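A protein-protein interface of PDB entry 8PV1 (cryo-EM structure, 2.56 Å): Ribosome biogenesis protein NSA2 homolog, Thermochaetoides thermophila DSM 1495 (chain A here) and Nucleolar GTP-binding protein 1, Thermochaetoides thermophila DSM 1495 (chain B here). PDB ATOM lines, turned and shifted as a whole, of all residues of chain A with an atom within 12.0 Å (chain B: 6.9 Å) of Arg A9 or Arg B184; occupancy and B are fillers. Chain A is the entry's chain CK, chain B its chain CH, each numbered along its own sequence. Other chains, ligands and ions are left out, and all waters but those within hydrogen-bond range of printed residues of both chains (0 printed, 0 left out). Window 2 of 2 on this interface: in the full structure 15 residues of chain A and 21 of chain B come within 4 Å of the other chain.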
ATOM      1  N   PRO A   2      18.800 -22.485  18.824  1.00  0.00           N
ATOM      2  CA  PRO A   2      17.584 -21.719  19.093  1.00  0.00           C
ATOM      3  C   PRO A   2      17.817 -20.702  20.200  1.00  0.00           C
ATOM      4  O   PRO A   2      18.763 -20.838  20.970  1.00  0.00           O
ATOM      5  CB  PRO A   2      16.590 -22.795  19.510  1.00  0.00           C
ATOM      6  CG  PRO A   2      17.426 -23.814  20.169  1.00  0.00           C
ATOM      7  CD  PRO A   2      18.763 -23.802  19.477  1.00  0.00           C
ATOM      8  N   GLN A   3      16.963 -19.688  20.275  1.00  0.00           N
ATOM      9  CA  GLN A   3      17.171 -18.581  21.192  1.00  0.00           C
ATOM     10  C   GLN A   3      15.836 -18.121  21.754  1.00  0.00           C
ATOM     11  O   GLN A   3      14.808 -18.181  21.074  1.00  0.00           O
ATOM     12  CB  GLN A   3      17.893 -17.425  20.490  1.00  0.00           C
ATOM     13  CG  GLN A   3      17.303 -17.075  19.135  1.00  0.00           C
ATOM     14  CD  GLN A   3      18.251 -16.272  18.269  1.00  0.00           C
ATOM     15  OE1 GLN A   3      19.278 -15.794  18.736  1.00  0.00           O
ATOM     16  NE2 GLN A   3      17.910 -16.129  16.997  1.00  0.00           N
ATOM     17  N   ASN A   4      15.871 -17.688  23.010  1.00  0.00           N
ATOM     18  CA  ASN A   4      14.740 -17.085  23.744  1.00  0.00           C
ATOM     19  C   ASN A   4      13.643 -18.148  23.880  1.00  0.00           C
ATOM     20  O   ASN A   4      13.949 -19.315  24.158  1.00  0.00           O
ATOM     21  CB  ASN A   4      14.322 -15.794  23.074  1.00  0.00           C
ATOM     22  CG  ASN A   4      15.489 -14.861  22.848  1.00  0.00           C
ATOM     23  OD1 ASN A   4      16.244 -14.562  23.769  1.00  0.00           O
ATOM     24  ND2 ASN A   4      15.654 -14.407  21.614  1.00  0.00           N
ATOM     25  N   GLU A   5      12.373 -17.794  23.701  1.00  0.00           N
ATOM     26  CA  GLU A   5      11.272 -18.722  23.958  1.00  0.00           C
ATOM     27  C   GLU A   5      10.965 -19.541  22.703  1.00  0.00           C
ATOM     28  O   GLU A   5       9.906 -19.432  22.082  1.00  0.00           O
ATOM     29  CB  GLU A   5      10.046 -17.964  24.447  1.00  0.00           C
ATOM     30  CG  GLU A   5      10.032 -17.726  25.944  1.00  0.00           C
ATOM     31  CD  GLU A   5      10.900 -16.558  26.361  1.00  0.00           C
ATOM     32  OE1 GLU A   5      11.287 -15.759  25.485  1.00  0.00           O
ATOM     33  OE2 GLU A   5      11.195 -16.438  27.568  1.00  0.00           O
ATOM     34  N   TYR A   6      11.924 -20.401  22.350  1.00  0.00           N
ATOM     35  CA  TYR A   6      11.810 -21.139  21.097  1.00  0.00           C
ATOM     36  C   TYR A   6      10.779 -22.256  21.191  1.00  0.00           C
ATOM     37  O   TYR A   6      10.104 -22.561  20.203  1.00  0.00           O
ATOM     38  CB  TYR A   6      13.171 -21.688  20.668  1.00  0.00           C
ATOM     39  CG  TYR A   6      13.945 -22.468  21.710  1.00  0.00           C
ATOM     40  CD1 TYR A   6      13.776 -23.841  21.847  1.00  0.00           C
ATOM     41  CD2 TYR A   6      14.889 -21.841  22.509  1.00  0.00           C
ATOM     42  CE1 TYR A   6      14.500 -24.559  22.777  1.00  0.00           C
ATOM     43  CE2 TYR A   6      15.618 -22.551  23.439  1.00  0.00           C
ATOM     44  CZ  TYR A   6      15.419 -23.909  23.570  1.00  0.00           C
ATOM     45  OH  TYR A   6      16.139 -24.623  24.498  1.00  0.00           O
ATOM     46  N   ILE A   7      10.628 -22.870  22.367  1.00  0.00           N
ATOM     47  CA  ILE A   7       9.601 -23.897  22.523  1.00  0.00           C
ATOM     48  C   ILE A   7       8.212 -23.272  22.461  1.00  0.00           C
ATOM     49  O   ILE A   7       7.290 -23.842  21.868  1.00  0.00           O
ATOM     50  CB  ILE A   7       9.832 -24.708  23.814  1.00  0.00           C
ATOM     51  CG1 ILE A   7      11.012 -25.670  23.637  1.00  0.00           C
ATOM     52  CG2 ILE A   7       8.604 -25.503  24.218  1.00  0.00           C
ATOM     53  CD1 ILE A   7      10.766 -26.755  22.613  1.00  0.00           C
ATOM     54  N   GLU A   8       8.048 -22.066  23.014  1.00  0.00           N
ATOM     55  CA  GLU A   8       6.773 -21.364  22.876  1.00  0.00           C
ATOM     56  C   GLU A   8       6.511 -20.942  21.436  1.00  0.00           C
ATOM     57  O   GLU A   8       5.367 -21.003  20.970  1.00  0.00           O
ATOM     58  CB  GLU A   8       6.718 -20.149  23.794  1.00  0.00           C
ATOM     59  CG  GLU A   8       6.695 -20.482  25.259  1.00  0.00           C
ATOM     60  CD  GLU A   8       6.871 -19.254  26.116  1.00  0.00           C
ATOM     61  OE1 GLU A   8       6.623 -18.140  25.607  1.00  0.00           O
ATOM     62  OE2 GLU A   8       7.265 -19.399  27.292  1.00  0.00           O
ATOM     63  N   ARG A   9       7.548 -20.514  20.714  1.00  0.00           N
ATOM     64  CA  ARG A   9       7.355 -20.174  19.306  1.00  0.00           C
ATOM     65  C   ARG A   9       6.977 -21.403  18.483  1.00  0.00           C
ATOM     66  O   ARG A   9       6.113 -21.323  17.601  1.00  0.00           O
ATOM     67  CB  ARG A   9       8.611 -19.513  18.744  1.00  0.00           C
ATOM     68  CG  ARG A   9       8.508 -19.166  17.266  1.00  0.00           C
ATOM     69  CD  ARG A   9       9.105 -17.799  16.971  1.00  0.00           C
ATOM     70  NE  ARG A   9       8.986 -17.418  15.568  1.00  0.00           N
ATOM     71  CZ  ARG A   9       7.905 -16.873  15.029  1.00  0.00           C
ATOM     72  NH1 ARG A   9       6.826 -16.620  15.751  1.00  0.00           N
ATOM     73  NH2 ARG A   9       7.908 -16.564  13.735  1.00  0.00           N
ATOM     74  N   HIS A  10       7.602 -22.551  18.765  1.00  0.00           N
ATOM     75  CA  HIS A  10       7.232 -23.789  18.083  1.00  0.00           C
ATOM     76  C   HIS A  10       5.811 -24.205  18.440  1.00  0.00           C
ATOM     77  O   HIS A  10       5.064 -24.689  17.583  1.00  0.00           O
ATOM     78  CB  HIS A  10       8.221 -24.903  18.430  1.00  0.00           C
ATOM     79  CG  HIS A  10       7.975 -26.177  17.685  1.00  0.00           C
ATOM     80  ND1 HIS A  10       8.483 -26.422  16.427  1.00  0.00           N
ATOM     81  CD2 HIS A  10       7.239 -27.265  18.009  1.00  0.00           C
ATOM     82  CE1 HIS A  10       8.087 -27.613  16.018  1.00  0.00           C
ATOM     83  NE2 HIS A  10       7.326 -28.143  16.958  1.00  0.00           N
ATOM     84  N   ARG A  11       5.424 -23.991  19.702  1.00  0.00           N
ATOM     85  CA  ARG A  11       4.081 -24.290  20.182  1.00  0.00           C
ATOM     86  C   ARG A  11       3.044 -23.452  19.449  1.00  0.00           C
ATOM     87  O   ARG A  11       1.972 -23.948  19.083  1.00  0.00           O
ATOM     88  CB  ARG A  11       4.037 -24.025  21.686  1.00  0.00           C
ATOM     89  CG  ARG A  11       2.700 -24.106  22.330  1.00  0.00           C
ATOM     90  CD  ARG A  11       2.865 -24.668  23.733  1.00  0.00           C
ATOM     91  NE  ARG A  11       3.947 -24.028  24.471  1.00  0.00           N
ATOM     92  CZ  ARG A  11       4.918 -24.668  25.110  1.00  0.00           C
ATOM     93  NH1 ARG A  11       5.023 -25.986  25.071  1.00  0.00           N
ATOM     94  NH2 ARG A  11       5.805 -23.966  25.810  1.00  0.00           N
ATOM     95  N   LYS A  12       3.373 -22.188  19.190  1.00  0.00           N
ATOM     96  CA  LYS A  12       2.461 -21.302  18.478  1.00  0.00           C
ATOM     97  C   LYS A  12       2.416 -21.620  16.984  1.00  0.00           C
ATOM     98  O   LYS A  12       1.363 -21.493  16.349  1.00  0.00           O
ATOM     99  CB  LYS A  12       2.884 -19.854  18.714  1.00  0.00           C
ATOM    100  CG  LYS A  12       2.693 -19.405  20.154  1.00  0.00           C
ATOM    101  CD  LYS A  12       3.110 -17.961  20.299  1.00  0.00           C
ATOM    102  CE  LYS A  12       2.969 -17.455  21.715  1.00  0.00           C
ATOM    103  NZ  LYS A  12       3.405 -16.031  21.805  1.00  0.00           N
ATOM    104  N   LEU A  13       3.539 -22.054  16.406  1.00  0.00           N
ATOM    105  CA  LEU A  13       3.591 -22.265  14.960  1.00  0.00           C
ATOM    106  C   LEU A  13       3.084 -23.635  14.522  1.00  0.00           C
ATOM    107  O   LEU A  13       2.646 -23.784  13.376  1.00  0.00           O
ATOM    108  CB  LEU A  13       5.017 -22.074  14.447  1.00  0.00           C
ATOM    109  CG  LEU A  13       5.597 -20.661  14.389  1.00  0.00           C
ATOM    110  CD1 LEU A  13       7.059 -20.723  14.013  1.00  0.00           C
ATOM    111  CD2 LEU A  13       4.840 -19.818  13.383  1.00  0.00           C
ATOM    112  N   HIS A  14       3.148 -24.641  15.394  1.00  0.00           N
ATOM    113  CA  HIS A  14       2.855 -26.016  15.016  1.00  0.00           C
ATOM    114  C   HIS A  14       1.866 -26.728  15.929  1.00  0.00           C
ATOM    115  O   HIS A  14       1.427 -27.832  15.585  1.00  0.00           O
ATOM    116  CB  HIS A  14       4.160 -26.826  14.952  1.00  0.00           C
ATOM    117  CG  HIS A  14       5.219 -26.191  14.106  1.00  0.00           C
ATOM    118  ND1 HIS A  14       6.238 -25.428  14.634  1.00  0.00           N
ATOM    119  CD2 HIS A  14       5.426 -26.221  12.769  1.00  0.00           C
ATOM    120  CE1 HIS A  14       7.019 -25.003  13.656  1.00  0.00           C
ATOM    121  NE2 HIS A  14       6.550 -25.474  12.515  1.00  0.00           N
ATOM    122  N   GLY A  15       1.501 -26.144  17.067  1.00  0.00           N
ATOM    123  CA  GLY A  15       0.565 -26.784  17.966  1.00  0.00           C
ATOM    124  C   GLY A  15       1.227 -27.855  18.813  1.00  0.00           C
ATOM    125  O   GLY A  15       2.445 -27.881  19.024  1.00  0.00           O
ATOM    126  N   ARG A  16       0.391 -28.766  19.293  1.00  0.00           N
ATOM    127  CA  ARG A  16       0.797 -29.863  20.152  1.00  0.00           C
ATOM    128  C   ARG A  16       0.994 -31.108  19.294  1.00  0.00           C
ATOM    129  O   ARG A  16       0.963 -31.055  18.064  1.00  0.00           O
ATOM    130  CB  ARG A  16      -0.283 -30.171  21.193  1.00  0.00           C
ATOM    131  CG  ARG A  16      -0.465 -29.259  22.382  1.00  0.00           C
ATOM    132  CD  ARG A  16      -1.373 -28.101  21.995  1.00  0.00           C
ATOM    133  NE  ARG A  16      -1.799 -27.318  23.147  1.00  0.00           N
ATOM    134  CZ  ARG A  16      -1.214 -26.227  23.613  1.00  0.00           C
ATOM    135  NH1 ARG A  16      -0.161 -25.700  23.015  1.00  0.00           N
ATOM    136  NH2 ARG A  16      -1.708 -25.648  24.704  1.00  0.00           N
ATOM    137  N   LYS B 179      13.033  -3.586  11.613  1.00  0.00           N
ATOM    138  CA  LYS B 179      14.292  -4.178  12.061  1.00  0.00           C
ATOM    139  C   LYS B 179      14.272  -5.697  11.936  1.00  0.00           C
ATOM    140  O   LYS B 179      15.183  -6.298  11.349  1.00  0.00           O
ATOM    141  CB  LYS B 179      14.572  -3.766  13.506  1.00  0.00           C
ATOM    142  CG  LYS B 179      14.587  -2.270  13.741  1.00  0.00           C
ATOM    143  CD  LYS B 179      15.019  -1.936  15.159  1.00  0.00           C
ATOM    144  CE  LYS B 179      14.109  -2.569  16.195  1.00  0.00           C
ATOM    145  NZ  LYS B 179      12.754  -1.959  16.202  1.00  0.00           N
ATOM    146  N   SER B 180      13.233  -6.335  12.478  1.00  0.00           N
ATOM    147  CA  SER B 180      13.135  -7.787  12.387  1.00  0.00           C
ATOM    148  C   SER B 180      12.883  -8.249  10.961  1.00  0.00           C
ATOM    149  O   SER B 180      13.317  -9.342  10.591  1.00  0.00           O
ATOM    150  CB  SER B 180      12.044  -8.311  13.316  1.00  0.00           C
ATOM    151  OG  SER B 180      12.381  -8.082  14.669  1.00  0.00           O
ATOM    152  N   SER B 181      12.198  -7.439  10.149  1.00  0.00           N
ATOM    153  CA  SER B 181      12.043  -7.774   8.737  1.00  0.00           C
ATOM    154  C   SER B 181      13.386  -7.791   8.018  1.00  0.00           C
ATOM    155  O   SER B 181      13.656  -8.708   7.230  1.00  0.00           O
ATOM    156  CB  SER B 181      11.092  -6.789   8.063  1.00  0.00           C
ATOM    157  OG  SER B 181       9.767  -6.964   8.527  1.00  0.00           O
ATOM    158  N   PHE B 182      14.246  -6.810   8.300  1.00  0.00           N
ATOM    159  CA  PHE B 182      15.581  -6.792   7.712  1.00  0.00           C
ATOM    160  C   PHE B 182      16.410  -7.984   8.181  1.00  0.00           C
ATOM    161  O   PHE B 182      17.119  -8.615   7.382  1.00  0.00           O
ATOM    162  CB  PHE B 182      16.280  -5.479   8.058  1.00  0.00           C
ATOM    163  CG  PHE B 182      17.672  -5.371   7.515  1.00  0.00           C
ATOM    164  CD1 PHE B 182      17.886  -5.140   6.167  1.00  0.00           C
ATOM    165  CD2 PHE B 182      18.768  -5.493   8.352  1.00  0.00           C
ATOM    166  CE1 PHE B 182      19.167  -5.038   5.665  1.00  0.00           C
ATOM    167  CE2 PHE B 182      20.050  -5.396   7.854  1.00  0.00           C
ATOM    168  CZ  PHE B 182      20.249  -5.167   6.509  1.00  0.00           C
ATOM    169  N   VAL B 183      16.330  -8.307   9.475  1.00  0.00           N
ATOM    170  CA  VAL B 183      17.118  -9.411  10.022  1.00  0.00           C
ATOM    171  C   VAL B 183      16.642 -10.749   9.459  1.00  0.00           C
ATOM    172  O   VAL B 183      17.455 -11.625   9.138  1.00  0.00           O
ATOM    173  CB  VAL B 183      17.084  -9.375  11.563  1.00  0.00           C
ATOM    174  CG1 VAL B 183      17.746 -10.604  12.160  1.00  0.00           C
ATOM    175  CG2 VAL B 183      17.794  -8.131  12.057  1.00  0.00           C
ATOM    176  N   ARG B 184      15.325 -10.918   9.299  1.00  0.00           N
ATOM    177  CA  ARG B 184      14.800 -12.105   8.633  1.00  0.00           C
ATOM    178  C   ARG B 184      15.235 -12.184   7.178  1.00  0.00           C
ATOM    179  O   ARG B 184      15.538 -13.275   6.685  1.00  0.00           O
ATOM    180  CB  ARG B 184      13.274 -12.137   8.702  1.00  0.00           C
ATOM    181  CG  ARG B 184      12.696 -12.493  10.051  1.00  0.00           C
ATOM    182  CD  ARG B 184      11.213 -12.786   9.921  1.00  0.00           C
ATOM    183  NE  ARG B 184      10.969 -14.103   9.348  1.00  0.00           N
ATOM    184  CZ  ARG B 184      10.790 -15.206  10.061  1.00  0.00           C
ATOM    185  NH1 ARG B 184      10.815 -15.186  11.383  1.00  0.00           N
ATOM    186  NH2 ARG B 184      10.578 -16.358   9.432  1.00  0.00           N
ATOM    187  N   SER B 185      15.263 -11.053   6.474  1.00  0.00           N
ATOM    188  CA  SER B 185      15.633 -11.074   5.067  1.00  0.00           C
ATOM    189  C   SER B 185      17.115 -11.342   4.835  1.00  0.00           C
ATOM    190  O   SER B 185      17.464 -11.895   3.788  1.00  0.00           O
ATOM    191  CB  SER B 185      15.241  -9.757   4.399  1.00  0.00           C
ATOM    192  OG  SER B 185      15.872  -8.658   5.028  1.00  0.00           O
ATOM    193  N   VAL B 186      17.994 -10.974   5.766  1.00  0.00           N
ATOM    194  CA  VAL B 186      19.428 -11.172   5.564  1.00  0.00           C
ATOM    195  C   VAL B 186      19.989 -12.371   6.313  1.00  0.00           C
ATOM    196  O   VAL B 186      21.096 -12.819   5.979  1.00  0.00           O
ATOM    197  CB  VAL B 186      20.240  -9.908   5.921  1.00  0.00           C
ATOM    198  CG1 VAL B 186      19.766  -8.721   5.103  1.00  0.00           C
ATOM    199  CG2 VAL B 186      20.191  -9.620   7.413  1.00  0.00           C
ATOM    200  N   THR B 187      19.288 -12.917   7.308  1.00  0.00           N
ATOM    201  CA  THR B 187      19.800 -14.043   8.080  1.00  0.00           C
ATOM    202  C   THR B 187      18.774 -15.168   8.081  1.00  0.00           C
ATOM    203  O   THR B 187      17.751 -15.112   7.390  1.00  0.00           O
ATOM    204  CB  THR B 187      20.139 -13.643   9.524  1.00  0.00           C
ATOM    205  OG1 THR B 187      18.955 -13.195  10.191  1.00  0.00           O
ATOM    206  CG2 THR B 187      21.195 -12.545   9.561  1.00  0.00           C
ATOM    207  N   ARG B 188      19.065 -16.203   8.863  1.00  0.00           N
ATOM    208  CA  ARG B 188      18.177 -17.340   9.052  1.00  0.00           C
ATOM    209  C   ARG B 188      17.524 -17.346  10.429  1.00  0.00           C
ATOM    210  O   ARG B 188      16.833 -18.311  10.770  1.00  0.00           O
ATOM    211  CB  ARG B 188      18.953 -18.645   8.829  1.00  0.00           C
ATOM    212  CG  ARG B 188      18.137 -19.787   8.241  1.00  0.00           C
ATOM    213  CD  ARG B 188      18.993 -21.025   8.024  1.00  0.00           C
ATOM    214  NE  ARG B 188      19.336 -21.687   9.279  1.00  0.00           N
ATOM    215  CZ  ARG B 188      18.543 -22.530   9.928  1.00  0.00           C
ATOM    216  NH1 ARG B 188      17.340 -22.837   9.473  1.00  0.00           N
ATOM    217  NH2 ARG B 188      18.969 -23.077  11.062  1.00  0.00           N
ATOM    218  N   ALA B 189      17.726 -16.295  11.223  1.00  0.00           N
ATOM    219  CA  ALA B 189      17.153 -16.231  12.560  1.00  0.00           C
ATOM    220  C   ALA B 189      15.638 -16.109  12.496  1.00  0.00           C
ATOM    221  O   ALA B 189      15.091 -15.437  11.617  1.00  0.00           O
ATOM    222  CB  ALA B 189      17.741 -15.050  13.330  1.00  0.00           C
ATOM    223  N   ASP B 190      14.959 -16.773  13.430  1.00  0.00           N
ATOM    224  CA  ASP B 190      13.498 -16.773  13.476  1.00  0.00           C
ATOM    225  C   ASP B 190      13.018 -15.733  14.489  1.00  0.00           C
ATOM    226  O   ASP B 190      12.456 -16.040  15.541  1.00  0.00           O
ATOM    227  CB  ASP B 190      12.980 -18.168  13.806  1.00  0.00           C
ATOM    228  CG  ASP B 190      11.474 -18.283  13.670  1.00  0.00           C
ATOM    229  OD1 ASP B 190      10.867 -17.434  12.984  1.00  0.00           O
ATOM    230  OD2 ASP B 190      10.896 -19.221  14.256  1.00  0.00           O
ATOM    231  N   THR B 191      13.266 -14.471  14.153  1.00  0.00           N
ATOM    232  CA  THR B 191      12.726 -13.365  14.931  1.00  0.00           C
ATOM    233  C   THR B 191      11.349 -12.989  14.392  1.00  0.00           C
ATOM    234  O   THR B 191      11.190 -12.855  13.172  1.00  0.00           O
ATOM    235  CB  THR B 191      13.680 -12.169  14.923  1.00  0.00           C
ATOM    236  OG1 THR B 191      13.082 -11.062  15.610  1.00  0.00           O
ATOM    237  CG2 THR B 191      14.121 -11.763  13.511  1.00  0.00           C
ATOM    238  N   PRO B 192      10.324 -12.900  15.237  1.00  0.00           N
ATOM    239  CA  PRO B 192       8.970 -12.637  14.731  1.00  0.00           C
ATOM    240  C   PRO B 192       8.824 -11.231  14.165  1.00  0.00           C
ATOM    241  O   PRO B 192       9.449 -10.280  14.637  1.00  0.00           O
ATOM    242  CB  PRO B 192       8.087 -12.835  15.967  1.00  0.00           C
ATOM    243  CG  PRO B 192       8.897 -13.685  16.884  1.00  0.00           C
ATOM    244  CD  PRO B 192      10.316 -13.277  16.660  1.00  0.00           C
ATOM    245  N   VAL B 193       7.978 -11.112  13.144  1.00  0.00           N
ATOM    246  CA  VAL B 193       7.634  -9.835  12.528  1.00  0.00           C
ATOM    247  C   VAL B 193       6.134  -9.640  12.695  1.00  0.00           C
ATOM    248  O   VAL B 193       5.339 -10.455  12.214  1.00  0.00           O
ATOM    249  CB  VAL B 193       8.038  -9.787  11.046  1.00  0.00           C
ATOM    250  CG1 VAL B 193       7.317  -8.659  10.327  1.00  0.00           C
ATOM    251  CG2 VAL B 193       9.535  -9.620  10.918  1.00  0.00           C
ATOM    252  N   GLU B 194       5.752  -8.577  13.389  1.00  0.00           N
ATOM    253  CA  GLU B 194       4.367  -8.309  13.744  1.00  0.00           C
ATOM    254  C   GLU B 194       4.124  -6.808  13.698  1.00  0.00           C
ATOM    255  O   GLU B 194       5.056  -6.020  13.891  1.00  0.00           O
ATOM    256  CB  GLU B 194       4.039  -8.855  15.140  1.00  0.00           C
ATOM    257  CG  GLU B 194       4.012 -10.374  15.270  1.00  0.00           C
ATOM    258  CD  GLU B 194       2.742 -10.991  14.718  1.00  0.00           C
ATOM    259  OE1 GLU B 194       1.776 -10.246  14.454  1.00  0.00           O
ATOM    260  OE2 GLU B 194       2.710 -12.228  14.546  1.00  0.00           O
ATOM    261  N   PHE B 204      18.069 -10.831  19.534  1.00  0.00           N
ATOM    262  CA  PHE B 204      18.136 -11.954  18.611  1.00  0.00           C
ATOM    263  C   PHE B 204      19.402 -11.818  17.781  1.00  0.00           C
ATOM    264  O   PHE B 204      19.886 -10.709  17.550  1.00  0.00           O
ATOM    265  CB  PHE B 204      16.920 -12.000  17.677  1.00  0.00           C
ATOM    266  CG  PHE B 204      15.684 -12.579  18.301  1.00  0.00           C
ATOM    267  CD1 PHE B 204      14.894 -11.816  19.144  1.00  0.00           C
ATOM    268  CD2 PHE B 204      15.297 -13.879  18.022  1.00  0.00           C
ATOM    269  CE1 PHE B 204      13.748 -12.343  19.710  1.00  0.00           C
ATOM    270  CE2 PHE B 204      14.154 -14.412  18.583  1.00  0.00           C
ATOM    271  CZ  PHE B 204      13.377 -13.643  19.426  1.00  0.00           C
ATOM    272  N   ASP B 219      19.392  -8.245  16.158  1.00  0.00           N
ATOM    273  CA  ASP B 219      18.098  -7.591  16.218  1.00  0.00           C
ATOM    274  C   ASP B 219      17.767  -7.253  17.666  1.00  0.00           C
ATOM    275  O   ASP B 219      17.927  -8.077  18.570  1.00  0.00           O
ATOM    276  CB  ASP B 219      17.016  -8.496  15.628  1.00  0.00           C
ATOM    277  CG  ASP B 219      15.667  -7.814  15.530  1.00  0.00           C
ATOM    278  OD1 ASP B 219      15.613  -6.568  15.575  1.00  0.00           O
ATOM    279  OD2 ASP B 219      14.656  -8.531  15.400  1.00  0.00           O
ATOM    280  N   GLN B 324      11.806  -6.262  -0.832  1.00  0.00           N
ATOM    281  CA  GLN B 324      13.202  -6.693  -0.798  1.00  0.00           C
ATOM    282  C   GLN B 324      14.117  -5.863  -1.689  1.00  0.00           C
ATOM    283  O   GLN B 324      15.192  -6.347  -2.062  1.00  0.00           O
ATOM    284  CB  GLN B 324      13.369  -8.176  -1.170  1.00  0.00           C
ATOM    285  CG  GLN B 324      12.731  -9.135  -0.185  1.00  0.00           C
ATOM    286  CD  GLN B 324      13.409  -9.108   1.166  1.00  0.00           C
ATOM    287  OE1 GLN B 324      14.626  -8.958   1.257  1.00  0.00           O
ATOM    288  NE2 GLN B 324      12.624  -9.253   2.227  1.00  0.00           N
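The side-chain carboxylate (OD2) of Asp B190 is in salt-bridge range of the guanidinium group (NE) of Arg A9 (2.9 Å).
The guanidinium group of Arg B184 sits at hydrogen-bond distance from the backbone carbonyl oxygen of Thr B191, 3.0 Å away. The guanidinium group of Arg B184 is in salt-bridge range of the side-chain carboxylate of Asp B190. OG1 of Thr B187 sits at hydrogen-bond distance from N of Ala B189, at 3.5 Å. The backbone carbonyl oxygen of Phe B204 is in hydrogen-bond range of the backbone NH of Asp B219, 2.9 Å away.
NE2 of Gln A3 touches CB of Ala B189, 3.8 Å away. Phe B204 touches Gln A3. Asn A4 touches Phe B204 (ND2 to CZ, 3.2 Å). Arg A9 touches Arg B184 (NH2 to NH1, 3.99 Å). NH1 of Arg A9 touches CG of Pro B192, 3.8 Å away.
Printed residues of chain B within 4 Å of Gln A3: Ala B189 (3.8 Å) and Phe B204 (3.6 Å). Of the printed residues of chain B, Asn A4 touches Phe B204 (3.2 Å). Of the printed residues of chain B, Arg A9 touches Arg B184, Asp B190 and Pro B192. No residue of chain A comes within 4 Å of Ser B181. Of the printed residues of chain A, Arg B184 touches Arg A9. No residue of chain A comes within 4 Å of Ser B185. No residue of chain A comes within 4 Å of Val B186. No residue of chain A comes within 4 Å of Thr B191. Of chain A, only Arg A9 comes within 4 Å of Pro B192. No residue of chain A comes within 4 Å of Val B193. The nearest printed residue of chain B that does not touch Arg A9 is Thr B191 (5.0 Å).
Printed residues of chain B that touch a printed residue of chain A: Arg B184, Ala B189, Asp B190, Pro B192 and Phe B204. Of the 15 printed residues of chain A, 3 touch a printed residue of chain B. Printed residues of chain A that touch a printed residue of chain B: Gln A3, Asn A4 and Arg A9. Among the printed residues, 6 pairs touch across the chains. Among the printed residues, Asp or Glu carboxylates within 4 Å of a Lys or Arg side-chain nitrogen of the other chain: Arg A9 with Asp B190 (2.9 Å).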
